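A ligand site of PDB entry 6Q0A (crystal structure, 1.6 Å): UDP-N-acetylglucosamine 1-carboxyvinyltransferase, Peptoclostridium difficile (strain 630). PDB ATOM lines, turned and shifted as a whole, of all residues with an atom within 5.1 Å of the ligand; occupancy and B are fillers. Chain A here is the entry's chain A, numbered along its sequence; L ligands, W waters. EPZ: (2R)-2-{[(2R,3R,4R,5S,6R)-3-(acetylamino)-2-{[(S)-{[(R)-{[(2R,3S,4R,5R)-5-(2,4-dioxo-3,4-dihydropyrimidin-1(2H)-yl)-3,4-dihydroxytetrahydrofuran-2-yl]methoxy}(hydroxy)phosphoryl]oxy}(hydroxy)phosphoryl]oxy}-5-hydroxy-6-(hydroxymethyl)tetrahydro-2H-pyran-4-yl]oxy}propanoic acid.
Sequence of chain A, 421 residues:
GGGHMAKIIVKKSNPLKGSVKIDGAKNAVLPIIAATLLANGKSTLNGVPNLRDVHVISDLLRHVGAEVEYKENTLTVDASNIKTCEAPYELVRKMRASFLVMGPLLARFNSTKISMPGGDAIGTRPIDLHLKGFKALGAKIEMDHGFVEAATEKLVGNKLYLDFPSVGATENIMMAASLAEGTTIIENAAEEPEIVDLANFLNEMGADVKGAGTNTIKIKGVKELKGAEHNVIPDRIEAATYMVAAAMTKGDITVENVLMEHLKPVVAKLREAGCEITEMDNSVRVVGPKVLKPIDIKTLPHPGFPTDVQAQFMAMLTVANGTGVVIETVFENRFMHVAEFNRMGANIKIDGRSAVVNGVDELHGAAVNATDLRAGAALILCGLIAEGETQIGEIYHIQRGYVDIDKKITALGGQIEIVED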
ATOM      1  N   LYS A  26     -29.698 -15.306  13.002  1.00  0.00           N
ATOM      2  CA  LYS A  26     -28.386 -14.651  13.176  1.00  0.00           C
ATOM      3  C   LYS A  26     -27.989 -14.635  14.648  1.00  0.00           C
ATOM      4  O   LYS A  26     -26.842 -14.965  14.984  1.00  0.00           O
ATOM      5  CB  LYS A  26     -28.408 -13.220  12.633  1.00  0.00           C
ATOM      6  CG  LYS A  26     -27.039 -12.565  12.710  1.00  0.00           C
ATOM      7  CD  LYS A  26     -26.971 -11.176  12.091  1.00  0.00           C
ATOM      8  CE  LYS A  26     -27.705 -10.121  12.894  1.00  0.00           C
ATOM      9  NZ  LYS A  26     -27.093  -9.820  14.207  1.00  0.00           N
ATOM     10  N   ASN A  27     -28.923 -14.235  15.530  1.00  0.00           N
ATOM     11  CA  ASN A  27     -28.565 -13.989  16.936  1.00  0.00           C
ATOM     12  C   ASN A  27     -28.554 -15.294  17.742  1.00  0.00           C
ATOM     13  O   ASN A  27     -28.053 -15.252  18.883  1.00  0.00           O
ATOM     14  CB  ASN A  27     -29.437 -12.883  17.506  1.00  0.00           C
ATOM     15  CG  ASN A  27     -28.999 -11.554  16.900  1.00  0.00           C
ATOM     16  OD1 ASN A  27     -27.945 -11.491  16.275  1.00  0.00           O
ATOM     17  ND2 ASN A  27     -29.741 -10.486  17.148  1.00  0.00           N
ATOM     18  N   LEU A  30     -24.621 -16.663  16.220  1.00  0.00           N
ATOM     19  CA  LEU A  30     -23.364 -15.988  16.574  1.00  0.00           C
ATOM     20  C   LEU A  30     -22.859 -16.492  17.913  1.00  0.00           C
ATOM     21  O   LEU A  30     -21.698 -16.839  18.040  1.00  0.00           O
ATOM     22  CB  LEU A  30     -23.515 -14.472  16.493  1.00  0.00           C
ATOM     23  CG  LEU A  30     -23.761 -13.911  15.088  1.00  0.00           C
ATOM     24  CD1 LEU A  30     -24.091 -12.434  15.151  1.00  0.00           C
ATOM     25  CD2 LEU A  30     -22.569 -14.125  14.186  1.00  0.00           C
ATOM     26  N   ARG A  96     -19.602  -6.306  16.812  1.00  0.00           N
ATOM     27  CA  ARG A  96     -19.372  -6.289  18.277  1.00  0.00           C
ATOM     28  C   ARG A  96     -19.691  -7.655  18.888  1.00  0.00           C
ATOM     29  O   ARG A  96     -19.165  -7.916  19.990  1.00  0.00           O
ATOM     30  CB  ARG A  96     -20.109  -5.155  18.987  1.00  0.00           C
ATOM     31  CG  ARG A  96     -21.610  -5.200  18.844  1.00  0.00           C
ATOM     32  CD  ARG A  96     -22.224  -4.025  19.607  1.00  0.00           C
ATOM     33  NE  ARG A  96     -22.180  -4.166  21.063  1.00  0.00           N
ATOM     34  CZ  ARG A  96     -21.587  -3.348  21.923  1.00  0.00           C
ATOM     35  NH1 ARG A  96     -20.969  -2.241  21.531  1.00  0.00           N
ATOM     36  NH2 ARG A  96     -21.650  -3.628  23.210  1.00  0.00           N
ATOM     37  N   ALA A  97     -20.442  -8.510  18.210  1.00  0.00           N
ATOM     38  CA  ALA A  97     -20.749  -9.879  18.718  1.00  0.00           C
ATOM     39  C   ALA A  97     -19.450 -10.697  18.809  1.00  0.00           C
ATOM     40  O   ALA A  97     -19.460 -11.772  19.487  1.00  0.00           O
ATOM     41  CB  ALA A  97     -21.829 -10.514  17.895  1.00  0.00           C
ATOM     42  N   LEU A 100     -18.347 -12.058  22.191  1.00  0.00           N
ATOM     43  CA  LEU A 100     -18.870 -13.339  22.764  1.00  0.00           C
ATOM     44  C   LEU A 100     -17.829 -14.450  22.749  1.00  0.00           C
ATOM     45  O   LEU A 100     -18.107 -15.492  23.305  1.00  0.00           O
ATOM     46  CB  LEU A 100     -20.108 -13.761  22.006  1.00  0.00           C
ATOM     47  CG  LEU A 100     -21.261 -12.780  22.082  1.00  0.00           C
ATOM     48  CD1 LEU A 100     -22.381 -13.208  21.160  1.00  0.00           C
ATOM     49  CD2 LEU A 100     -21.743 -12.626  23.537  1.00  0.00           C
ATOM     50  N   ILE A 122     -26.802   2.257  17.709  1.00  0.00           N
ATOM     51  CA  ILE A 122     -28.086   2.271  18.453  1.00  0.00           C
ATOM     52  C   ILE A 122     -27.887   2.589  19.930  1.00  0.00           C
ATOM     53  O   ILE A 122     -28.902   2.625  20.660  1.00  0.00           O
ATOM     54  CB  ILE A 122     -28.856   0.971  18.270  1.00  0.00           C
ATOM     55  CG1 ILE A 122     -28.136  -0.209  18.902  1.00  0.00           C
ATOM     56  CG2 ILE A 122     -29.174   0.731  16.791  1.00  0.00           C
ATOM     57  CD1 ILE A 122     -28.931  -1.484  18.808  1.00  0.00           C
ATOM     58  N   ARG A 125     -23.700   1.071  24.806  1.00  0.00           N
ATOM     59  CA  ARG A 125     -23.653  -0.411  24.880  1.00  0.00           C
ATOM     60  C   ARG A 125     -22.410  -0.885  25.639  1.00  0.00           C
ATOM     61  O   ARG A 125     -21.542  -1.544  25.054  1.00  0.00           O
ATOM     62  CB  ARG A 125     -23.773  -1.013  23.496  1.00  0.00           C
ATOM     63  CG  ARG A 125     -25.100  -0.659  22.829  1.00  0.00           C
ATOM     64  CD  ARG A 125     -25.273  -1.329  21.497  1.00  0.00           C
ATOM     65  NE  ARG A 125     -25.447  -2.790  21.572  1.00  0.00           N
ATOM     66  CZ  ARG A 125     -25.592  -3.561  20.520  1.00  0.00           C
ATOM     67  NH1 ARG A 125     -25.768  -4.872  20.660  1.00  0.00           N
ATOM     68  NH2 ARG A 125     -25.625  -3.037  19.298  1.00  0.00           N
ATOM     69  N   PRO A 126     -22.338  -0.611  26.948  1.00  0.00           N
ATOM     70  CA  PRO A 126     -21.198  -1.086  27.747  1.00  0.00           C
ATOM     71  C   PRO A 126     -21.257  -2.602  27.916  1.00  0.00           C
ATOM     72  O   PRO A 126     -22.296  -3.201  27.674  1.00  0.00           O
ATOM     73  CB  PRO A 126     -21.345  -0.382  29.081  1.00  0.00           C
ATOM     74  CG  PRO A 126     -22.792  -0.068  29.196  1.00  0.00           C
ATOM     75  CD  PRO A 126     -23.321   0.084  27.780  1.00  0.00           C
ATOM     76  N   ILE A 127     -20.107  -3.177  28.333  1.00  0.00           N
ATOM     77  CA  ILE A 127     -20.023  -4.634  28.564  1.00  0.00           C
ATOM     78  C   ILE A 127     -19.660  -4.920  30.029  1.00  0.00           C
ATOM     79  O   ILE A 127     -19.244  -6.048  30.336  1.00  0.00           O
ATOM     80  CB  ILE A 127     -19.059  -5.290  27.537  1.00  0.00           C
ATOM     81  CG1 ILE A 127     -17.703  -4.607  27.411  1.00  0.00           C
ATOM     82  CG2 ILE A 127     -19.724  -5.367  26.175  1.00  0.00           C
ATOM     83  CD1 ILE A 127     -16.853  -4.579  28.666  1.00  0.00           C
ATOM     84  N   ASP A 128     -19.962  -3.974  30.926  1.00  0.00           N
ATOM     85  CA  ASP A 128     -19.702  -4.075  32.377  1.00  0.00           C
ATOM     86  C   ASP A 128     -20.292  -5.354  32.976  1.00  0.00           C
ATOM     87  O   ASP A 128     -19.725  -5.926  33.914  1.00  0.00           O
ATOM     88  CB  ASP A 128     -20.255  -2.851  33.110  1.00  0.00           C
ATOM     89  CG  ASP A 128     -21.769  -2.642  32.951  1.00  0.00           C
ATOM     90  OD1 ASP A 128     -22.467  -2.666  33.956  1.00  0.00           O
ATOM     91  OD2 ASP A 128     -22.223  -2.417  31.796  1.00  0.00           O
ATOM     92  N   LEU A 129     -21.483  -5.803  32.544  1.00  0.00           N
ATOM     93  CA  LEU A 129     -22.135  -6.966  33.185  1.00  0.00           C
ATOM     94  C   LEU A 129     -21.414  -8.234  32.781  1.00  0.00           C
ATOM     95  O   LEU A 129     -21.443  -9.185  33.530  1.00  0.00           O
ATOM     96  CB  LEU A 129     -23.611  -7.015  32.800  1.00  0.00           C
ATOM     97  CG  LEU A 129     -24.453  -5.876  33.347  1.00  0.00           C
ATOM     98  CD1 LEU A 129     -25.864  -5.953  32.802  1.00  0.00           C
ATOM     99  CD2 LEU A 129     -24.486  -5.946  34.882  1.00  0.00           C
ATOM    100  N   HIS A 130     -20.803  -8.252  31.586  1.00  0.00           N
ATOM    101  CA  HIS A 130     -19.973  -9.409  31.209  1.00  0.00           C
ATOM    102  C   HIS A 130     -18.804  -9.529  32.198  1.00  0.00           C
ATOM    103  O   HIS A 130     -18.583 -10.651  32.740  1.00  0.00           O
ATOM    104  CB  HIS A 130     -19.404  -9.276  29.790  1.00  0.00           C
ATOM    105  CG  HIS A 130     -20.424  -9.137  28.715  1.00  0.00           C
ATOM    106  ND1 HIS A 130     -20.463 -10.005  27.646  1.00  0.00           N
ATOM    107  CD2 HIS A 130     -21.417  -8.242  28.512  1.00  0.00           C
ATOM    108  CE1 HIS A 130     -21.434  -9.628  26.827  1.00  0.00           C
ATOM    109  NE2 HIS A 130     -22.044  -8.545  27.339  1.00  0.00           N
ATOM    110  N   PHE A 164     -29.276  -5.954  34.758  1.00  0.00           N
ATOM    111  CA  PHE A 164     -30.219  -5.955  33.618  1.00  0.00           C
ATOM    112  C   PHE A 164     -30.066  -7.317  32.969  1.00  0.00           C
ATOM    113  O   PHE A 164     -28.943  -7.851  32.947  1.00  0.00           O
ATOM    114  CB  PHE A 164     -29.902  -4.814  32.670  1.00  0.00           C
ATOM    115  CG  PHE A 164     -30.922  -4.616  31.581  1.00  0.00           C
ATOM    116  CD1 PHE A 164     -32.029  -3.816  31.804  1.00  0.00           C
ATOM    117  CD2 PHE A 164     -30.782  -5.253  30.365  1.00  0.00           C
ATOM    118  CE1 PHE A 164     -33.012  -3.689  30.832  1.00  0.00           C
ATOM    119  CE2 PHE A 164     -31.772  -5.116  29.385  1.00  0.00           C
ATOM    120  CZ  PHE A 164     -32.855  -4.299  29.610  1.00  0.00           C
ATOM    121  N   PRO A 165     -31.166  -7.873  32.438  1.00  0.00           N
ATOM    122  CA  PRO A 165     -31.133  -9.226  31.889  1.00  0.00           C
ATOM    123  C   PRO A 165     -30.513  -9.209  30.494  1.00  0.00           C
ATOM    124  O   PRO A 165     -31.218  -9.440  29.487  1.00  0.00           O
ATOM    125  CB  PRO A 165     -32.587  -9.704  31.925  1.00  0.00           C
ATOM    126  CG  PRO A 165     -33.392  -8.415  31.830  1.00  0.00           C
ATOM    127  CD  PRO A 165     -32.541  -7.393  32.567  1.00  0.00           C
ATOM    128  N   SER A 166     -29.241  -8.847  30.480  1.00  0.00           N
ATOM    129  CA  SER A 166     -28.452  -8.692  29.237  1.00  0.00           C
ATOM    130  C   SER A 166     -28.356 -10.024  28.516  1.00  0.00           C
ATOM    131  O   SER A 166     -27.876 -11.048  29.081  1.00  0.00           O
ATOM    132  CB  SER A 166     -27.082  -8.130  29.546  1.00  0.00           C
ATOM    133  OG  SER A 166     -26.184  -8.358  28.452  1.00  0.00           O
ATOM    134  N   VAL A 167     -28.731  -9.999  27.237  1.00  0.00           N
ATOM    135  CA  VAL A 167     -28.550 -11.180  26.356  1.00  0.00           C
ATOM    136  C   VAL A 167     -27.061 -11.573  26.314  1.00  0.00           C
ATOM    137  O   VAL A 167     -26.692 -12.733  26.631  1.00  0.00           O
ATOM    138  CB  VAL A 167     -29.123 -10.867  24.961  1.00  0.00           C
ATOM    139  CG1 VAL A 167     -28.746 -11.881  23.921  1.00  0.00           C
ATOM    140  CG2 VAL A 167     -30.632 -10.662  25.019  1.00  0.00           C
ATOM    141  N   GLY A 168     -26.208 -10.639  25.927  1.00  0.00           N
ATOM    142  CA  GLY A 168     -24.785 -10.930  25.728  1.00  0.00           C
ATOM    143  C   GLY A 168     -24.125 -11.369  27.026  1.00  0.00           C
ATOM    144  O   GLY A 168     -23.324 -12.286  26.998  1.00  0.00           O
ATOM    145  N   ALA A 169     -24.424 -10.704  28.123  1.00  0.00           N
ATOM    146  CA  ALA A 169     -23.742 -11.068  29.396  1.00  0.00           C
ATOM    147  C   ALA A 169     -24.183 -12.461  29.814  1.00  0.00           C
ATOM    148  O   ALA A 169     -23.372 -13.257  30.277  1.00  0.00           O
ATOM    149  CB  ALA A 169     -24.075 -10.077  30.459  1.00  0.00           C
ATOM    150  N   GLU A 171     -25.069 -14.864  27.813  1.00  0.00           N
ATOM    151  CA  GLU A 171     -24.425 -15.846  26.918  1.00  0.00           C
ATOM    152  C   GLU A 171     -22.972 -16.033  27.352  1.00  0.00           C
ATOM    153  O   GLU A 171     -22.462 -17.155  27.475  1.00  0.00           O
ATOM    154  CB  GLU A 171     -24.478 -15.388  25.460  1.00  0.00           C
ATOM    155  CG  GLU A 171     -25.895 -15.381  24.930  1.00  0.00           C
ATOM    156  CD  GLU A 171     -26.208 -14.587  23.687  1.00  0.00           C
ATOM    157  OE1 GLU A 171     -25.461 -13.675  23.342  1.00  0.00           O
ATOM    158  OE2 GLU A 171     -27.283 -14.887  23.105  1.00  0.00           O
ATOM    159  N   GLU A 192     -34.463 -14.597  26.451  1.00  0.00           N
ATOM    160  CA  GLU A 192     -34.570 -14.684  24.963  1.00  0.00           C
ATOM    161  C   GLU A 192     -34.384 -16.115  24.453  1.00  0.00           C
ATOM    162  O   GLU A 192     -33.590 -16.943  24.972  1.00  0.00           O
ATOM    163  CB  GLU A 192     -33.577 -13.779  24.259  1.00  0.00           C
ATOM    164  CG  GLU A 192     -34.054 -12.343  24.077  1.00  0.00           C
ATOM    165  CD  GLU A 192     -34.171 -11.442  25.314  1.00  0.00           C
ATOM    166  OE1 GLU A 192     -33.685 -11.820  26.413  1.00  0.00           O
ATOM    167  OE2 GLU A 192     -34.765 -10.357  25.202  1.00  0.00           O
ATOM    168  N   THR A 307     -36.990  -5.046  20.939  1.00  0.00           N
ATOM    169  CA  THR A 307     -36.400  -3.808  20.424  1.00  0.00           C
ATOM    170  C   THR A 307     -36.001  -4.023  18.961  1.00  0.00           C
ATOM    171  O   THR A 307     -36.075  -3.088  18.217  1.00  0.00           O
ATOM    172  CB  THR A 307     -35.220  -3.323  21.301  1.00  0.00           C
ATOM    173  OG1 THR A 307     -34.625  -2.174  20.721  1.00  0.00           O
ATOM    174  CG2 THR A 307     -34.168  -4.384  21.532  1.00  0.00           C
ATOM    175  N   ASP A 308     -35.721  -5.258  18.573  1.00  0.00           N
ATOM    176  CA  ASP A 308     -35.284  -5.522  17.173  1.00  0.00           C
ATOM    177  C   ASP A 308     -36.462  -5.430  16.196  1.00  0.00           C
ATOM    178  O   ASP A 308     -36.189  -5.505  14.986  1.00  0.00           O
ATOM    179  CB  ASP A 308     -34.640  -6.900  17.024  1.00  0.00           C
ATOM    180  CG  ASP A 308     -33.216  -6.935  17.578  1.00  0.00           C
ATOM    181  OD1 ASP A 308     -32.750  -8.024  17.850  1.00  0.00           O
ATOM    182  OD2 ASP A 308     -32.612  -5.825  17.686  1.00  0.00           O
ATOM    183  N   VAL A 330     -34.967  -0.435  26.019  1.00  0.00           N
ATOM    184  CA  VAL A 330     -33.843  -1.408  25.983  1.00  0.00           C
ATOM    185  C   VAL A 330     -32.594  -0.686  25.475  1.00  0.00           C
ATOM    186  O   VAL A 330     -31.537  -0.843  26.120  1.00  0.00           O
ATOM    187  CB  VAL A 330     -34.160  -2.658  25.139  1.00  0.00           C
ATOM    188  CG1 VAL A 330     -32.917  -3.552  25.045  1.00  0.00           C
ATOM    189  CG2 VAL A 330     -35.331  -3.426  25.688  1.00  0.00           C
ATOM    190  N   PHE A 331     -32.676   0.108  24.408  1.00  0.00           N
ATOM    191  CA  PHE A 331     -31.511   0.796  23.861  1.00  0.00           C
ATOM    192  C   PHE A 331     -31.578   2.298  24.091  1.00  0.00           C
ATOM    193  O   PHE A 331     -32.648   2.828  24.313  1.00  0.00           O
ATOM    194  CB  PHE A 331     -31.287   0.423  22.409  1.00  0.00           C
ATOM    195  CG  PHE A 331     -30.556  -0.887  22.331  1.00  0.00           C
ATOM    196  CD1 PHE A 331     -29.234  -0.984  22.765  1.00  0.00           C
ATOM    197  CD2 PHE A 331     -31.177  -2.045  21.899  1.00  0.00           C
ATOM    198  CE1 PHE A 331     -28.575  -2.198  22.727  1.00  0.00           C
ATOM    199  CE2 PHE A 331     -30.511  -3.250  21.851  1.00  0.00           C
ATOM    200  CZ  PHE A 331     -29.204  -3.319  22.256  1.00  0.00           C
ATOM    201  N   GLU A 332     -30.417   2.976  24.116  1.00  0.00           N
ATOM    202  CA  GLU A 332     -30.448   4.424  24.446  1.00  0.00           C
ATOM    203  C   GLU A 332     -31.021   5.124  23.215  1.00  0.00           C
ATOM    204  O   GLU A 332     -32.163   5.597  23.224  1.00  0.00           O
ATOM    205  CB  GLU A 332     -29.051   4.941  24.835  1.00  0.00           C
ATOM    206  CG  GLU A 332     -29.110   5.990  25.931  1.00  0.00           C
ATOM    207  CD  GLU A 332     -29.419   5.462  27.322  1.00  0.00           C
ATOM    208  OE1 GLU A 332     -30.172   6.136  28.072  1.00  0.00           O
ATOM    209  OE2 GLU A 332     -28.898   4.366  27.671  1.00  0.00           O
ATOM    210  N   ARG A 334     -32.122   4.418  20.066  1.00  0.00           N
ATOM    211  CA  ARG A 334     -32.532   3.606  18.885  1.00  0.00           C
ATOM    212  C   ARG A 334     -33.670   4.331  18.132  1.00  0.00           C
ATOM    213  O   ARG A 334     -34.603   3.701  17.760  1.00  0.00           O
ATOM    214  CB  ARG A 334     -32.883   2.177  19.276  1.00  0.00           C
ATOM    215  CG  ARG A 334     -32.745   1.201  18.108  1.00  0.00           C
ATOM    216  CD  ARG A 334     -32.992  -0.217  18.545  1.00  0.00           C
ATOM    217  NE  ARG A 334     -32.682  -1.128  17.434  1.00  0.00           N
ATOM    218  CZ  ARG A 334     -32.606  -2.449  17.530  1.00  0.00           C
ATOM    219  NH1 ARG A 334     -32.855  -3.036  18.678  1.00  0.00           N
ATOM    220  NH2 ARG A 334     -32.179  -3.144  16.493  1.00  0.00           N
ATOM    221  N   LEU A 373     -29.234  -2.280  11.042  1.00  0.00           N
ATOM    222  CA  LEU A 373     -29.851  -3.479  10.447  1.00  0.00           C
ATOM    223  C   LEU A 373     -31.380  -3.404  10.420  1.00  0.00           C
ATOM    224  O   LEU A 373     -31.987  -3.522   9.369  1.00  0.00           O
ATOM    225  CB  LEU A 373     -29.365  -4.684  11.268  1.00  0.00           C
ATOM    226  CG  LEU A 373     -30.056  -6.009  10.972  1.00  0.00           C
ATOM    227  CD1 LEU A 373     -29.960  -6.429   9.490  1.00  0.00           C
ATOM    228  CD2 LEU A 373     -29.452  -7.095  11.825  1.00  0.00           C
ATOM    229  N   ARG A 374     -31.993  -3.168  11.564  1.00  0.00           N
ATOM    230  CA  ARG A 374     -33.451  -3.337  11.628  1.00  0.00           C
ATOM    231  C   ARG A 374     -34.139  -2.103  11.056  1.00  0.00           C
ATOM    232  O   ARG A 374     -35.222  -2.247  10.410  1.00  0.00           O
ATOM    233  CB  ARG A 374     -33.887  -3.658  13.071  1.00  0.00           C
ATOM    234  CG  ARG A 374     -33.197  -4.868  13.676  1.00  0.00           C
ATOM    235  CD  ARG A 374     -33.419  -6.147  12.868  1.00  0.00           C
ATOM    236  NE  ARG A 374     -32.713  -7.299  13.385  1.00  0.00           N
ATOM    237  CZ  ARG A 374     -32.576  -8.463  12.756  1.00  0.00           C
ATOM    238  NH1 ARG A 374     -33.144  -8.645  11.561  1.00  0.00           N
ATOM    239  NH2 ARG A 374     -31.851  -9.399  13.313  1.00  0.00           N
HETATM  240  C1  EPZ L   1     -28.390  -8.715  21.546  1.00  0.00           C
HETATM  241  O1  EPZ L   1     -27.512  -7.638  21.854  1.00  0.00           O
HETATM  242  C2  EPZ L   1     -28.541  -8.771  20.020  1.00  0.00           C
HETATM  243  N2  EPZ L   1     -27.288  -9.152  19.397  1.00  0.00           N
HETATM  244  C3  EPZ L   1     -29.098  -7.433  19.530  1.00  0.00           C
HETATM  245  O3  EPZ L   1     -29.223  -7.410  18.092  1.00  0.00           O
HETATM  246  C4  EPZ L   1     -30.451  -7.193  20.213  1.00  0.00           C
HETATM  247  O4  EPZ L   1     -30.986  -5.939  19.807  1.00  0.00           O
HETATM  248  C5  EPZ L   1     -30.212  -7.203  21.715  1.00  0.00           C
HETATM  249  O5  EPZ L   1     -29.664  -8.477  22.135  1.00  0.00           O
HETATM  250  C6  EPZ L   1     -31.457  -7.008  22.571  1.00  0.00           C
HETATM  251  O6  EPZ L   1     -32.533  -7.897  22.156  1.00  0.00           O
HETATM  252  C7  EPZ L   1     -26.927 -10.416  19.359  1.00  0.00           C
HETATM  253  O7  EPZ L   1     -27.632 -11.310  19.817  1.00  0.00           O
HETATM  254  C8  EPZ L   1     -25.544 -10.685  18.803  1.00  0.00           C
HETATM  255  PA  EPZ L   1     -28.113  -6.728  25.671  1.00  0.00           P
HETATM  256  PB  EPZ L   1     -26.729  -7.515  23.227  1.00  0.00           P
HETATM  257  O1A EPZ L   1     -29.302  -7.516  26.124  1.00  0.00           O
HETATM  258  O1B EPZ L   1     -26.465  -8.868  23.762  1.00  0.00           O
HETATM  259  C1D EPZ L   1     -27.241  -2.814  28.274  1.00  0.00           C
HETATM  260  C1E EPZ L   1     -27.920  -6.942  16.086  1.00  0.00           C
HETATM  261  O1E EPZ L   1     -26.981  -6.277  15.595  1.00  0.00           O
HETATM  262  N1U EPZ L   1     -26.066  -3.563  28.784  1.00  0.00           N
HETATM  263  O2A EPZ L   1     -26.796  -7.046  26.286  1.00  0.00           O
HETATM  264  O2B EPZ L   1     -25.699  -6.466  23.064  1.00  0.00           O
HETATM  265  C2D EPZ L   1     -27.069  -2.440  26.807  1.00  0.00           C
HETATM  266  O2D EPZ L   1     -26.336  -1.245  26.588  1.00  0.00           O
HETATM  267  C2E EPZ L   1     -28.335  -6.470  17.468  1.00  0.00           C
HETATM  268  O2E EPZ L   1     -28.530  -7.899  15.567  1.00  0.00           O
HETATM  269  C2U EPZ L   1     -25.294  -2.978  29.773  1.00  0.00           C
HETATM  270  O2U EPZ L   1     -25.577  -1.907  30.308  1.00  0.00           O
HETATM  271  O3A EPZ L   1     -27.894  -6.889  24.119  1.00  0.00           O
HETATM  272  C3D EPZ L   1     -28.543  -2.277  26.401  1.00  0.00           C
HETATM  273  O3D EPZ L   1     -29.048  -0.996  26.744  1.00  0.00           O
HETATM  274  C3E EPZ L   1     -28.985  -5.112  17.368  1.00  0.00           C
HETATM  275  N3U EPZ L   1     -24.210  -3.719  30.168  1.00  0.00           N
HETATM  276  C4D EPZ L   1     -29.219  -3.377  27.199  1.00  0.00           C
HETATM  277  O4D EPZ L   1     -28.341  -3.684  28.323  1.00  0.00           O
HETATM  278  C4U EPZ L   1     -23.794  -4.937  29.661  1.00  0.00           C
HETATM  279  O4U EPZ L   1     -22.752  -5.451  30.113  1.00  0.00           O
HETATM  280  C5D EPZ L   1     -29.503  -4.652  26.445  1.00  0.00           C
HETATM  281  O5D EPZ L   1     -28.287  -5.139  25.832  1.00  0.00           O
HETATM  282  C5U EPZ L   1     -24.616  -5.452  28.609  1.00  0.00           C
HETATM  283  C6U EPZ L   1     -25.702  -4.762  28.211  1.00  0.00           C
HETATM  284  O   HOH W   1     -31.087  -7.906  15.627  1.00  0.00           O
HETATM  285  O   HOH W   2     -25.336  -4.777  16.975  1.00  0.00           O
HETATM  286  O   HOH W   3     -32.092  -7.264  26.373  1.00  0.00           O
HETATM  287  O   HOH W   4     -24.028  -7.321  25.741  1.00  0.00           O
HETATM  288  O   HOH W   5     -24.694  -7.176  18.767  1.00  0.00           O
HETATM  289  O   HOH W   6     -32.287 -10.530  21.206  1.00  0.00           O
HETATM  290  O   HOH W   7     -34.797  -7.689  20.261  1.00  0.00           O
HETATM  291  O   HOH W   8     -25.595  -4.045  24.096  1.00  0.00           O
HETATM  292  O   HOH W   9     -26.217  -5.048  13.138  1.00  0.00           O
HETATM  293  O   HOH W  10     -28.211 -13.617  20.999  1.00  0.00           O
HETATM  294  O   HOH W  11     -34.003  -7.796  24.554  1.00  0.00           O
HETATM  295  O   HOH W  12     -25.159 -10.715  22.367  1.00  0.00           O
HETATM  296  O   HOH W  13     -27.534   1.418  25.005  1.00  0.00           O
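The backbone carbonyl oxygen of Val 330 is in hydrogen-bond range of an oxygen (O3D) of the ligand (2.6 Å).
The side-chain hydroxyl of Ser 166 sits at hydrogen-bond distance from an oxygen (O2A) of the ligand (2.6 Å).
An oxygen (O4) of the ligand lies within hydrogen-bond range of the side-chain carboxylate (OD2) of Asp 308.
The side-chain amino group (NZ) of Lys 26 lies within salt-bridge range of an oxygen (O2E) of the ligand (2.8 Å).
O4U of the ligand lies within hydrogen-bond range of N of Leu 129 (2.8 Å).
An oxygen (O1A) of the ligand lies within hydrogen-bond range of the backbone NH of Val 167 (2.8 Å).
O1B of the ligand is in hydrogen-bond range of N of Gly 168 (2.8 Å).
An oxygen (O4U) of the ligand sits at hydrogen-bond distance from the backbone NH (N) of Asp 128 (3.3 Å).
N3U of the ligand is in hydrogen-bond range of OD2 of Asp 128 (2.9 Å).
An oxygen (O2B) of the ligand is in salt-bridge range of the guanidinium group (NH1) of Arg 125 (2.9 Å).
N3U of the ligand sits close to O of Pro 126 (3.2 Å).
ND2 of Asn 27 lies within hydrogen-bond range of O3 of the ligand, 3.3 Å away.
The backbone NH (N) of Gly 168 lies within hydrogen-bond range of the side-chain hydroxyl (OG) of Ser 166 (3.4 Å).
The side-chain hydroxyl (OG) of Ser 166 is in hydrogen-bond range of the backbone NH (N) of Ala 169 (3.0 Å).
The side-chain carboxylate (OD2) of Asp 308 lies within salt-bridge range of the guanidinium group (NH2) of Arg 334 (3.0 Å).
The side-chain amide oxygen (OD1) of Asn 27 sits at hydrogen-bond distance from the side-chain amino group (NZ) of Lys 26.
The backbone carbonyl oxygen of Arg 125 is in hydrogen-bond range of the guanidinium group of Arg 96, at 2.8 Å.
The backbone NH (N) of Ala 169 sits at hydrogen-bond distance from a ring nitrogen (NE2) of His 130 (3.3 Å).
OG1 of Thr 307 lies within hydrogen-bond range of NH1 of Arg 334 (2.8 Å).
Merely in contact with the ligand: Ile 127 (3.1 Å), Phe 331 (3.4 Å), His 130 (3.5 Å), Phe 164 (3.5 Å), Arg 334 (3.6 Å), Ala 97 (3.8 Å), Ile 122 (3.9 Å), Thr 307 (3.9 Å) and Leu 373 (3.9 Å).
Hydrophobic or aromatic side chains within 4 Å of the ligand: Ala 97, Ile 122, Pro 126, Leu 129, His 130, Phe 164, Val 167, Val 330, Phe 331 and Leu 373.
Within 4 Å of the ligand: Lys 26, Asn 27, Ala 97, Ile 122, Arg 125, Pro 126, Ile 127, Asp 128, Leu 129, His 130, Phe 164, Ser 166, Val 167, Gly 168, Thr 307, Asp 308, Val 330, Phe 331, Arg 334 and Leu 373.
Along chain A the residues within 4 Å of the ligand span positions 26 to 373.
The nearest printed residue that does not touch the ligand is Arg 374 (4.3 Å).
Water W1 lies within hydrogen-bond range of an oxygen (O2E) of the ligand (2.6 Å), the side-chain carboxylate (OD1) of Asp 308 (2.8 Å), the guanidinium group (NE) of Arg 374 (2.8 Å) and the side-chain amide nitrogen (ND2) of Asn 27 (3.3 Å).
Water W2 bridges O1E of the ligand (2.6 Å) and NH2 of Arg 125 (2.9 Å).
Water W8 lies within hydrogen-bond range of an oxygen (O2B) of the ligand (2.6 Å) and the guanidinium group of Arg 125 (2.8 Å).
Water W11 bridges the side-chain carboxylate of Glu 192 and an oxygen (O6) of the ligand.
Water W4 lies within hydrogen-bond range of NE2 of His 130 (2.8 Å) and O2A of the ligand (2.8 Å).
Water W13 lies within hydrogen-bond range of an oxygen (O2D) of the ligand (3.3 Å) and the backbone NH (N) of Glu 332 (3.4 Å).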
